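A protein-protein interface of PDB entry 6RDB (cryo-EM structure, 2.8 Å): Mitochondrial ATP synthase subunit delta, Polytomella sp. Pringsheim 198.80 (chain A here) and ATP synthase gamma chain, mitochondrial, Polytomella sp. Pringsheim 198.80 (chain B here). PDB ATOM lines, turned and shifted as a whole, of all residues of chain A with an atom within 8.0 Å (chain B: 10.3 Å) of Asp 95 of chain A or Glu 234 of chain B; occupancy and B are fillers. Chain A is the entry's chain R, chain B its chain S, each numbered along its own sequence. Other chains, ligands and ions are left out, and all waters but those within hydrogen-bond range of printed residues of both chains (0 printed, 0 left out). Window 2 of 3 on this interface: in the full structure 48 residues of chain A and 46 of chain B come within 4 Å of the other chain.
N of Ile 108 of chain A sits at hydrogen-bond distance from O of Asp 232 of chain B (3.0 Å).
The backbone NH (N) of Asp 232 of chain B sits at hydrogen-bond distance from the backbone carbonyl oxygen (O) of Pro 106 of chain A.
The side-chain carboxylate of Glu 234 of chain B sits at hydrogen-bond distance from the backbone NH of Val 94 of chain A (3.5 Å).
The backbone carbonyl oxygen (O) of Ile 108 of chain A lies within hydrogen-bond range of the backbone NH (N) of Glu 234 of chain B (3.0 Å).
O of Gln 110 of chain A lies close to OE1 of Glu 234 of chain B, at 3.4 Å.
The backbone NH of Asp 95 of chain A sits at hydrogen-bond distance from the side-chain carboxylate of Glu 234 of chain B, 3.1 Å away.
O of Phe 98 of chain A lies within hydrogen-bond range of N of Leu 91 of chain A (2.8 Å).
The backbone NH (N) of Val 94 of chain A is in hydrogen-bond range of the backbone carbonyl oxygen (O) of Gln 110 of chain A.
The backbone carbonyl oxygen (O) of Ala 109 of chain A is in hydrogen-bond range of the backbone NH (N) of Ala 134 of chain A (2.8 Å).
Among the printed residues, merely in contact across the chains: Gly 93 of chain A with Glu 234 of chain B (3.4 Å), Val 94 of chain A with Ala 235 of chain B (3.7 Å), Val 94 of chain A with Ser 236 of chain B (3.7 Å), Phe 98 of chain A with Glu 234 of chain B (3.8 Å), Pro 106 of chain A with Ala 230 of chain B (3.2 Å), Pro 106 of chain A with Tyr 231 of chain B (3.3 Å), Thr 107 of chain A with Tyr 231 of chain B (3.7 Å), Thr 107 of chain A with Asp 232 of chain B (3.4 Å), Ile 108 of chain A with Tyr 231 of chain B (3.7 Å), Ile 108 of chain A with Ile 233 of chain B (3.7 Å), Ala 109 of chain A with Glu 234 of chain B (3.3 Å), Gln 110 of chain A with Ala 235 of chain B (3.9 Å), Gln 110 of chain A with Val 242 of chain B (3.96 Å), Phe 133 of chain A with Val 242 of chain B (3.6 Å), Phe 133 of chain A with Asp 245 of chain B (3.7 Å) and Phe 133 of chain A with Leu 246 of chain B (3.5 Å).
Asp 95 of chain A touches just one residue of chain B: Glu 234.
Glu 234 of chain B touches just these residues of chain A: Gly 93 (3.4 Å), Val 94 (3.3 Å), Asp 95 (3.1 Å), Phe 98 (3.8 Å), Ile 108 (3.0 Å), Ala 109 (3.3 Å) and Gln 110 (3.4 Å).
Val 94 of chain A touches just these residues of chain B: Glu 234, Ala 235 and Ser 236.
Gly 96 of chain A touches none of the printed residues of chain B.
Ala 109 of chain A touches just one residue of chain B: Glu 234.
Of the printed residues of chain A, Ser 236 of chain B touches Val 94.
Of the printed residues of chain A, Asp 232 of chain B touches Pro 106 (2.6 Å), Thr 107 (3.4 Å) and Ile 108 (3.0 Å).
Printed residues of chain B within 4 Å of Phe 98 of chain A: Glu 234 (3.8 Å).
Of the printed residues of chain A, Val 242 of chain B touches Gln 110 and Phe 133.
Leu 91 of chain A touches none of the printed residues of chain B.
Lys 112 of chain A touches none of the printed residues of chain B.
The nearest residue of chain A that does not touch Glu 234 of chain B is Gly 96 of chain A (4.1 Å).
The nearest printed residue of chain B that does not touch Ile 108 of chain A is Leu 246 of chain B (4.03 Å).
Of the 16 printed residues of chain B, 10 touch a printed residue of chain A.
Printed residues of chain B that touch a printed residue of chain A: Ala 230, Tyr 231, Asp 232, Ile 233, Glu 234, Ala 235, Ser 236, Val 242, Asp 245 and Leu 246.
Hydrophobic or aromatic side chains of chain B that line the printed part of chain A: Tyr 231, Ala 235, Val 242 and Leu 246.
Printed residues of chain A that touch a printed residue of chain B: Gly 93, Val 94, Asp 95, Phe 98, Pro 106, Thr 107, Ile 108, Ala 109, Gln 110 and Phe 133.
Hydrophobic or aromatic side chains of chain A that line the printed part of chain B: Val 94, Phe 98, Pro 106, Ile 108, Ala 109 and Phe 133.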
ATOM      1  N   LEU A  91       2.628  15.763  14.171  1.00  0.00           N
ATOM      2  CA  LEU A  91       3.528  15.948  15.293  1.00  0.00           C
ATOM      3  C   LEU A  91       4.785  16.694  14.869  1.00  0.00           C
ATOM      4  O   LEU A  91       5.334  16.417  13.799  1.00  0.00           O
ATOM      5  CB  LEU A  91       3.919  14.598  15.894  1.00  0.00           C
ATOM      6  CG  LEU A  91       2.798  13.919  16.669  1.00  0.00           C
ATOM      7  CD1 LEU A  91       3.126  12.474  16.931  1.00  0.00           C
ATOM      8  CD2 LEU A  91       2.593  14.653  17.965  1.00  0.00           C
ATOM      9  N   PRO A  92       5.259  17.642  15.670  1.00  0.00           N
ATOM     10  CA  PRO A  92       6.475  18.414  15.329  1.00  0.00           C
ATOM     11  C   PRO A  92       7.790  17.833  15.852  1.00  0.00           C
ATOM     12  O   PRO A  92       8.389  18.317  16.806  1.00  0.00           O
ATOM     13  CB  PRO A  92       6.185  19.774  15.963  1.00  0.00           C
ATOM     14  CG  PRO A  92       5.353  19.443  17.159  1.00  0.00           C
ATOM     15  CD  PRO A  92       4.572  18.197  16.847  1.00  0.00           C
ATOM     16  N   GLY A  93       8.267  16.775  15.194  1.00  0.00           N
ATOM     17  CA  GLY A  93       9.494  16.117  15.603  1.00  0.00           C
ATOM     18  C   GLY A  93      10.728  16.974  15.396  1.00  0.00           C
ATOM     19  O   GLY A  93      10.698  18.018  14.748  1.00  0.00           O
ATOM     20  N   VAL A  94      11.843  16.526  15.979  1.00  0.00           N
ATOM     21  CA  VAL A  94      13.080  17.287  15.843  1.00  0.00           C
ATOM     22  C   VAL A  94      13.687  17.136  14.457  1.00  0.00           C
ATOM     23  O   VAL A  94      14.485  17.982  14.041  1.00  0.00           O
ATOM     24  CB  VAL A  94      14.110  16.903  16.920  1.00  0.00           C
ATOM     25  CG1 VAL A  94      13.575  17.215  18.293  1.00  0.00           C
ATOM     26  CG2 VAL A  94      14.475  15.444  16.816  1.00  0.00           C
ATOM     27  N   ASP A  95      13.337  16.077  13.727  1.00  0.00           N
ATOM     28  CA  ASP A  95      13.725  15.995  12.330  1.00  0.00           C
ATOM     29  C   ASP A  95      12.816  16.835  11.454  1.00  0.00           C
ATOM     30  O   ASP A  95      13.227  17.252  10.368  1.00  0.00           O
ATOM     31  CB  ASP A  95      13.704  14.542  11.859  1.00  0.00           C
ATOM     32  CG  ASP A  95      14.617  13.652  12.675  1.00  0.00           C
ATOM     33  OD1 ASP A  95      14.377  12.427  12.711  1.00  0.00           O
ATOM     34  OD2 ASP A  95      15.573  14.177  13.284  1.00  0.00           O
ATOM     35  N   GLY A  96      11.613  17.108  11.919  1.00  0.00           N
ATOM     36  CA  GLY A  96      10.630  17.837  11.149  1.00  0.00           C
ATOM     37  C   GLY A  96       9.244  17.335  11.488  1.00  0.00           C
ATOM     38  O   GLY A  96       9.072  16.392  12.250  1.00  0.00           O
ATOM     39  N   TYR A  97       8.254  17.996  10.900  1.00  0.00           N
ATOM     40  CA  TYR A  97       6.862  17.617  11.105  1.00  0.00           C
ATOM     41  C   TYR A  97       6.586  16.280  10.439  1.00  0.00           C
ATOM     42  O   TYR A  97       6.953  16.073   9.280  1.00  0.00           O
ATOM     43  CB  TYR A  97       5.933  18.686  10.542  1.00  0.00           C
ATOM     44  CG  TYR A  97       5.743  19.877  11.440  1.00  0.00           C
ATOM     45  CD1 TYR A  97       6.704  20.875  11.513  1.00  0.00           C
ATOM     46  CD2 TYR A  97       4.602  20.007  12.212  1.00  0.00           C
ATOM     47  CE1 TYR A  97       6.537  21.967  12.335  1.00  0.00           C
ATOM     48  CE2 TYR A  97       4.423  21.094  13.036  1.00  0.00           C
ATOM     49  CZ  TYR A  97       5.393  22.071  13.093  1.00  0.00           C
ATOM     50  OH  TYR A  97       5.217  23.158  13.913  1.00  0.00           O
ATOM     51  N   PHE A  98       5.968  15.363  11.169  1.00  0.00           N
ATOM     52  CA  PHE A  98       5.482  14.129  10.578  1.00  0.00           C
ATOM     53  C   PHE A  98       4.025  13.919  10.953  1.00  0.00           C
ATOM     54  O   PHE A  98       3.468  14.616  11.799  1.00  0.00           O
ATOM     55  CB  PHE A  98       6.335  12.920  10.986  1.00  0.00           C
ATOM     56  CG  PHE A  98       6.312  12.593  12.448  1.00  0.00           C
ATOM     57  CD1 PHE A  98       7.119  13.275  13.340  1.00  0.00           C
ATOM     58  CD2 PHE A  98       5.532  11.553  12.921  1.00  0.00           C
ATOM     59  CE1 PHE A  98       7.115  12.960  14.672  1.00  0.00           C
ATOM     60  CE2 PHE A  98       5.527  11.231  14.255  1.00  0.00           C
ATOM     61  CZ  PHE A  98       6.316  11.937  15.128  1.00  0.00           C
ATOM     62  N   PRO A 106       6.035   1.623  15.276  1.00  0.00           N
ATOM     63  CA  PRO A 106       6.348   2.064  16.639  1.00  0.00           C
ATOM     64  C   PRO A 106       7.460   3.102  16.661  1.00  0.00           C
ATOM     65  O   PRO A 106       8.473   2.976  15.970  1.00  0.00           O
ATOM     66  CB  PRO A 106       6.758   0.770  17.342  1.00  0.00           C
ATOM     67  CG  PRO A 106       5.990  -0.273  16.640  1.00  0.00           C
ATOM     68  CD  PRO A 106       5.849   0.163  15.211  1.00  0.00           C
ATOM     69  N   THR A 107       7.238   4.154  17.447  1.00  0.00           N
ATOM     70  CA  THR A 107       8.016   5.381  17.357  1.00  0.00           C
ATOM     71  C   THR A 107       8.099   6.014  18.735  1.00  0.00           C
ATOM     72  O   THR A 107       7.085   6.115  19.426  1.00  0.00           O
ATOM     73  CB  THR A 107       7.366   6.349  16.357  1.00  0.00           C
ATOM     74  OG1 THR A 107       7.425   5.789  15.041  1.00  0.00           O
ATOM     75  CG2 THR A 107       8.065   7.695  16.338  1.00  0.00           C
ATOM     76  N   ILE A 108       9.302   6.398  19.141  1.00  0.00           N
ATOM     77  CA  ILE A 108       9.520   7.289  20.274  1.00  0.00           C
ATOM     78  C   ILE A 108      10.091   8.571  19.692  1.00  0.00           C
ATOM     79  O   ILE A 108      11.276   8.637  19.348  1.00  0.00           O
ATOM     80  CB  ILE A 108      10.457   6.683  21.320  1.00  0.00           C
ATOM     81  CG1 ILE A 108       9.861   5.402  21.886  1.00  0.00           C
ATOM     82  CG2 ILE A 108      10.715   7.674  22.437  1.00  0.00           C
ATOM     83  CD1 ILE A 108      10.802   4.654  22.791  1.00  0.00           C
ATOM     84  N   ALA A 109       9.260   9.592  19.562  1.00  0.00           N
ATOM     85  CA  ALA A 109       9.626  10.802  18.845  1.00  0.00           C
ATOM     86  C   ALA A 109       9.779  11.952  19.823  1.00  0.00           C
ATOM     87  O   ALA A 109       8.817  12.325  20.495  1.00  0.00           O
ATOM     88  CB  ALA A 109       8.575  11.138  17.793  1.00  0.00           C
ATOM     89  N   GLN A 110      10.982  12.507  19.900  1.00  0.00           N
ATOM     90  CA  GLN A 110      11.192  13.738  20.644  1.00  0.00           C
ATOM     91  C   GLN A 110      10.733  14.908  19.795  1.00  0.00           C
ATOM     92  O   GLN A 110      11.099  15.010  18.623  1.00  0.00           O
ATOM     93  CB  GLN A 110      12.659  13.902  21.023  1.00  0.00           C
ATOM     94  CG  GLN A 110      12.966  15.216  21.720  1.00  0.00           C
ATOM     95  CD  GLN A 110      14.402  15.317  22.178  1.00  0.00           C
ATOM     96  OE1 GLN A 110      15.082  14.308  22.357  1.00  0.00           O
ATOM     97  NE2 GLN A 110      14.874  16.541  22.372  1.00  0.00           N
ATOM     98  N   LEU A 111       9.924  15.784  20.376  1.00  0.00           N
ATOM     99  CA  LEU A 111       9.308  16.866  19.629  1.00  0.00           C
ATOM    100  C   LEU A 111       9.972  18.201  19.941  1.00  0.00           C
ATOM    101  O   LEU A 111      10.351  18.469  21.083  1.00  0.00           O
ATOM    102  CB  LEU A 111       7.815  16.945  19.927  1.00  0.00           C
ATOM    103  CG  LEU A 111       7.011  15.664  19.708  1.00  0.00           C
ATOM    104  CD1 LEU A 111       5.552  15.919  20.003  1.00  0.00           C
ATOM    105  CD2 LEU A 111       7.181  15.135  18.314  1.00  0.00           C
ATOM    106  N   LYS A 112      10.111  19.029  18.909  1.00  0.00           N
ATOM    107  CA  LYS A 112      10.494  20.421  19.055  1.00  0.00           C
ATOM    108  C   LYS A 112       9.314  21.226  19.579  1.00  0.00           C
ATOM    109  O   LYS A 112       8.191  20.724  19.651  1.00  0.00           O
ATOM    110  CB  LYS A 112      10.947  20.988  17.710  1.00  0.00           C
ATOM    111  CG  LYS A 112      12.348  20.638  17.299  1.00  0.00           C
ATOM    112  CD  LYS A 112      12.550  20.971  15.833  1.00  0.00           C
ATOM    113  CE  LYS A 112      12.519  22.459  15.565  1.00  0.00           C
ATOM    114  NZ  LYS A 112      12.801  22.726  14.128  1.00  0.00           N
ATOM    115  N   PHE A 133       7.959  14.435  24.401  1.00  0.00           N
ATOM    116  CA  PHE A 133       7.972  13.273  23.532  1.00  0.00           C
ATOM    117  C   PHE A 133       6.568  12.861  23.109  1.00  0.00           C
ATOM    118  O   PHE A 133       5.565  13.277  23.687  1.00  0.00           O
ATOM    119  CB  PHE A 133       8.666  12.106  24.228  1.00  0.00           C
ATOM    120  CG  PHE A 133      10.036  12.438  24.737  1.00  0.00           C
ATOM    121  CD1 PHE A 133      11.139  12.268  23.929  1.00  0.00           C
ATOM    122  CD2 PHE A 133      10.222  12.912  26.024  1.00  0.00           C
ATOM    123  CE1 PHE A 133      12.398  12.577  24.386  1.00  0.00           C
ATOM    124  CE2 PHE A 133      11.474  13.212  26.485  1.00  0.00           C
ATOM    125  CZ  PHE A 133      12.565  13.049  25.664  1.00  0.00           C
ATOM    126  N   ALA A 134       6.514  12.041  22.062  1.00  0.00           N
ATOM    127  CA  ALA A 134       5.271  11.488  21.544  1.00  0.00           C
ATOM    128  C   ALA A 134       5.540  10.054  21.131  1.00  0.00           C
ATOM    129  O   ALA A 134       6.370   9.811  20.253  1.00  0.00           O
ATOM    130  CB  ALA A 134       4.749  12.295  20.358  1.00  0.00           C
ATOM    131  N   LEU B 228      12.381  -2.907  23.340  1.00  0.00           N
ATOM    132  CA  LEU B 228      12.567  -1.503  23.020  1.00  0.00           C
ATOM    133  C   LEU B 228      12.971  -1.283  21.572  1.00  0.00           C
ATOM    134  O   LEU B 228      12.812  -0.171  21.061  1.00  0.00           O
ATOM    135  CB  LEU B 228      13.629  -0.901  23.948  1.00  0.00           C
ATOM    136  CG  LEU B 228      13.781   0.609  24.087  1.00  0.00           C
ATOM    137  CD1 LEU B 228      12.580   1.182  24.800  1.00  0.00           C
ATOM    138  CD2 LEU B 228      15.049   0.902  24.854  1.00  0.00           C
ATOM    139  N   ALA B 230      11.427  -2.285  19.028  1.00  0.00           N
ATOM    140  CA  ALA B 230      10.279  -2.095  18.154  1.00  0.00           C
ATOM    141  C   ALA B 230      10.150  -0.644  17.716  1.00  0.00           C
ATOM    142  O   ALA B 230       9.694  -0.372  16.601  1.00  0.00           O
ATOM    143  CB  ALA B 230       9.002  -2.551  18.856  1.00  0.00           C
ATOM    144  N   TYR B 231      10.592   0.287  18.554  1.00  0.00           N
ATOM    145  CA  TYR B 231      10.335   1.704  18.357  1.00  0.00           C
ATOM    146  C   TYR B 231      11.427   2.348  17.521  1.00  0.00           C
ATOM    147  O   TYR B 231      12.618   2.134  17.763  1.00  0.00           O
ATOM    148  CB  TYR B 231      10.243   2.420  19.704  1.00  0.00           C
ATOM    149  CG  TYR B 231       9.181   1.877  20.627  1.00  0.00           C
ATOM    150  CD1 TYR B 231       7.872   2.320  20.543  1.00  0.00           C
ATOM    151  CD2 TYR B 231       9.494   0.932  21.589  1.00  0.00           C
ATOM    152  CE1 TYR B 231       6.904   1.832  21.385  1.00  0.00           C
ATOM    153  CE2 TYR B 231       8.533   0.438  22.432  1.00  0.00           C
ATOM    154  CZ  TYR B 231       7.240   0.891  22.326  1.00  0.00           C
ATOM    155  OH  TYR B 231       6.280   0.396  23.173  1.00  0.00           O
ATOM    156  N   ASP B 232      11.017   3.152  16.549  1.00  0.00           N
ATOM    157  CA  ASP B 232      11.945   3.986  15.800  1.00  0.00           C
ATOM    158  C   ASP B 232      12.218   5.253  16.592  1.00  0.00           C
ATOM    159  O   ASP B 232      11.296   6.015  16.890  1.00  0.00           O
ATOM    160  CB  ASP B 232      11.398   4.327  14.417  1.00  0.00           C
ATOM    161  CG  ASP B 232      11.551   3.191  13.441  1.00  0.00           C
ATOM    162  OD1 ASP B 232      12.509   2.406  13.601  1.00  0.00           O
ATOM    163  OD2 ASP B 232      10.725   3.088  12.513  1.00  0.00           O
ATOM    164  N   ILE B 233      13.481   5.473  16.931  1.00  0.00           N
ATOM    165  CA  ILE B 233      13.870   6.665  17.672  1.00  0.00           C
ATOM    166  C   ILE B 233      13.895   7.837  16.703  1.00  0.00           C
ATOM    167  O   ILE B 233      14.479   7.747  15.619  1.00  0.00           O
ATOM    168  CB  ILE B 233      15.233   6.478  18.349  1.00  0.00           C
ATOM    169  CG1 ILE B 233      15.269   5.159  19.120  1.00  0.00           C
ATOM    170  CG2 ILE B 233      15.522   7.644  19.275  1.00  0.00           C
ATOM    171  CD1 ILE B 233      14.254   5.070  20.226  1.00  0.00           C
ATOM    172  N   GLU B 234      13.251   8.930  17.084  1.00  0.00           N
ATOM    173  CA  GLU B 234      13.181  10.135  16.271  1.00  0.00           C
ATOM    174  C   GLU B 234      13.783  11.304  17.048  1.00  0.00           C
ATOM    175  O   GLU B 234      13.218  12.388  17.130  1.00  0.00           O
ATOM    176  CB  GLU B 234      11.737  10.387  15.835  1.00  0.00           C
ATOM    177  CG  GLU B 234      11.502  11.270  14.598  1.00  0.00           C
ATOM    178  CD  GLU B 234      11.202  12.719  14.925  1.00  0.00           C
ATOM    179  OE1 GLU B 234      10.628  12.985  15.996  1.00  0.00           O
ATOM    180  OE2 GLU B 234      11.545  13.598  14.116  1.00  0.00           O
ATOM    181  N   ALA B 235      14.930  11.077  17.672  1.00  0.00           N
ATOM    182  CA  ALA B 235      15.603  12.114  18.432  1.00  0.00           C
ATOM    183  C   ALA B 235      16.797  12.642  17.654  1.00  0.00           C
ATOM    184  O   ALA B 235      17.153  12.136  16.590  1.00  0.00           O
ATOM    185  CB  ALA B 235      16.043  11.585  19.795  1.00  0.00           C
ATOM    186  N   SER B 236      17.417  13.687  18.199  1.00  0.00           N
ATOM    187  CA  SER B 236      18.640  14.221  17.613  1.00  0.00           C
ATOM    188  C   SER B 236      19.794  13.248  17.795  1.00  0.00           C
ATOM    189  O   SER B 236      20.476  12.883  16.832  1.00  0.00           O
ATOM    190  CB  SER B 236      18.983  15.566  18.251  1.00  0.00           C
ATOM    191  OG  SER B 236      18.163  16.603  17.745  1.00  0.00           O
ATOM    192  N   HIS B 237      20.026  12.831  19.021  1.00  0.00           N
ATOM    193  CA  HIS B 237      21.115  11.950  19.384  1.00  0.00           C
ATOM    194  C   HIS B 237      20.585  10.541  19.637  1.00  0.00           C
ATOM    195  O   HIS B 237      19.471  10.195  19.240  1.00  0.00           O
ATOM    196  CB  HIS B 237      21.873  12.566  20.551  1.00  0.00           C
ATOM    197  CG  HIS B 237      22.576  13.831  20.179  1.00  0.00           C
ATOM    198  ND1 HIS B 237      21.912  15.025  19.999  1.00  0.00           N
ATOM    199  CD2 HIS B 237      23.878  14.082  19.909  1.00  0.00           C
ATOM    200  CE1 HIS B 237      22.776  15.960  19.650  1.00  0.00           C
ATOM    201  NE2 HIS B 237      23.977  15.415  19.593  1.00  0.00           N
ATOM    202  N   GLU B 238      21.414   9.704  20.253  1.00  0.00           N
ATOM    203  CA  GLU B 238      21.237   8.258  20.243  1.00  0.00           C
ATOM    204  C   GLU B 238      20.045   7.819  21.090  1.00  0.00           C
ATOM    205  O   GLU B 238      19.339   8.619  21.708  1.00  0.00           O
ATOM    206  CB  GLU B 238      22.499   7.567  20.749  1.00  0.00           C
ATOM    207  CG  GLU B 238      23.795   8.090  20.160  1.00  0.00           C
ATOM    208  CD  GLU B 238      23.711   8.299  18.667  1.00  0.00           C
ATOM    209  OE1 GLU B 238      23.852   9.462  18.232  1.00  0.00           O
ATOM    210  OE2 GLU B 238      23.484   7.310  17.941  1.00  0.00           O
ATOM    211  N   ARG B 239      19.821   6.508  21.106  1.00  0.00           N
ATOM    212  CA  ARG B 239      18.840   5.945  22.020  1.00  0.00           C
ATOM    213  C   ARG B 239      19.328   6.001  23.461  1.00  0.00           C
ATOM    214  O   ARG B 239      18.515   6.083  24.387  1.00  0.00           O
ATOM    215  CB  ARG B 239      18.509   4.512  21.610  1.00  0.00           C
ATOM    216  CG  ARG B 239      17.262   3.966  22.265  1.00  0.00           C
ATOM    217  CD  ARG B 239      16.916   2.604  21.743  1.00  0.00           C
ATOM    218  NE  ARG B 239      17.930   1.612  22.065  1.00  0.00           N
ATOM    219  CZ  ARG B 239      17.862   0.348  21.676  1.00  0.00           C
ATOM    220  NH1 ARG B 239      16.829  -0.063  20.958  1.00  0.00           N
ATOM    221  NH2 ARG B 239      18.820  -0.505  21.999  1.00  0.00           N
ATOM    222  N   ASP B 241      20.906   8.426  24.992  1.00  0.00           N
ATOM    223  CA  ASP B 241      20.672   9.721  25.612  1.00  0.00           C
ATOM    224  C   ASP B 241      19.314  10.329  25.290  1.00  0.00           C
ATOM    225  O   ASP B 241      19.037  11.441  25.748  1.00  0.00           O
ATOM    226  CB  ASP B 241      21.794  10.710  25.251  1.00  0.00           C
ATOM    227  CG  ASP B 241      22.122  10.726  23.781  1.00  0.00           C
ATOM    228  OD1 ASP B 241      21.402  10.088  23.000  1.00  0.00           O
ATOM    229  OD2 ASP B 241      23.130  11.358  23.407  1.00  0.00           O
ATOM    230  N   VAL B 242      18.462   9.646  24.523  1.00  0.00           N
ATOM    231  CA  VAL B 242      17.057  10.036  24.552  1.00  0.00           C
ATOM    232  C   VAL B 242      16.375   9.364  25.738  1.00  0.00           C
ATOM    233  O   VAL B 242      15.480   9.952  26.349  1.00  0.00           O
ATOM    234  CB  VAL B 242      16.340   9.750  23.212  1.00  0.00           C
ATOM    235  CG1 VAL B 242      16.146   8.278  22.948  1.00  0.00           C
ATOM    236  CG2 VAL B 242      15.005  10.436  23.162  1.00  0.00           C
ATOM    237  N   LEU B 243      16.831   8.170  26.134  1.00  0.00           N
ATOM    238  CA  LEU B 243      16.328   7.539  27.347  1.00  0.00           C
ATOM    239  C   LEU B 243      16.869   8.224  28.587  1.00  0.00           C
ATOM    240  O   LEU B 243      16.250   8.152  29.651  1.00  0.00           O
ATOM    241  CB  LEU B 243      16.691   6.057  27.368  1.00  0.00           C
ATOM    242  CG  LEU B 243      15.610   5.052  26.984  1.00  0.00           C
ATOM    243  CD1 LEU B 243      15.238   5.182  25.530  1.00  0.00           C
ATOM    244  CD2 LEU B 243      16.100   3.655  27.269  1.00  0.00           C
ATOM    245  N   ASP B 245      17.019  11.453  28.615  1.00  0.00           N
ATOM    246  CA  ASP B 245      16.023  12.511  28.714  1.00  0.00           C
ATOM    247  C   ASP B 245      14.668  11.988  29.161  1.00  0.00           C
ATOM    248  O   ASP B 245      13.899  12.738  29.767  1.00  0.00           O
ATOM    249  CB  ASP B 245      15.864  13.226  27.370  1.00  0.00           C
ATOM    250  CG  ASP B 245      17.113  13.976  26.949  1.00  0.00           C
ATOM    251  OD1 ASP B 245      17.972  14.252  27.811  1.00  0.00           O
ATOM    252  OD2 ASP B 245      17.228  14.300  25.750  1.00  0.00           O
ATOM    253  N   LEU B 246      14.368  10.723  28.891  1.00  0.00           N
ATOM    254  CA  LEU B 246      13.015  10.201  29.015  1.00  0.00           C
ATOM    255  C   LEU B 246      12.714   9.618  30.387  1.00  0.00           C
ATOM    256  O   LEU B 246      11.546   9.569  30.780  1.00  0.00           O
ATOM    257  CB  LEU B 246      12.781   9.158  27.920  1.00  0.00           C
ATOM    258  CG  LEU B 246      11.413   8.563  27.640  1.00  0.00           C
ATOM    259  CD1 LEU B 246      10.466   9.670  27.411  1.00  0.00           C
ATOM    260  CD2 LEU B 246      11.490   7.731  26.390  1.00  0.00           C
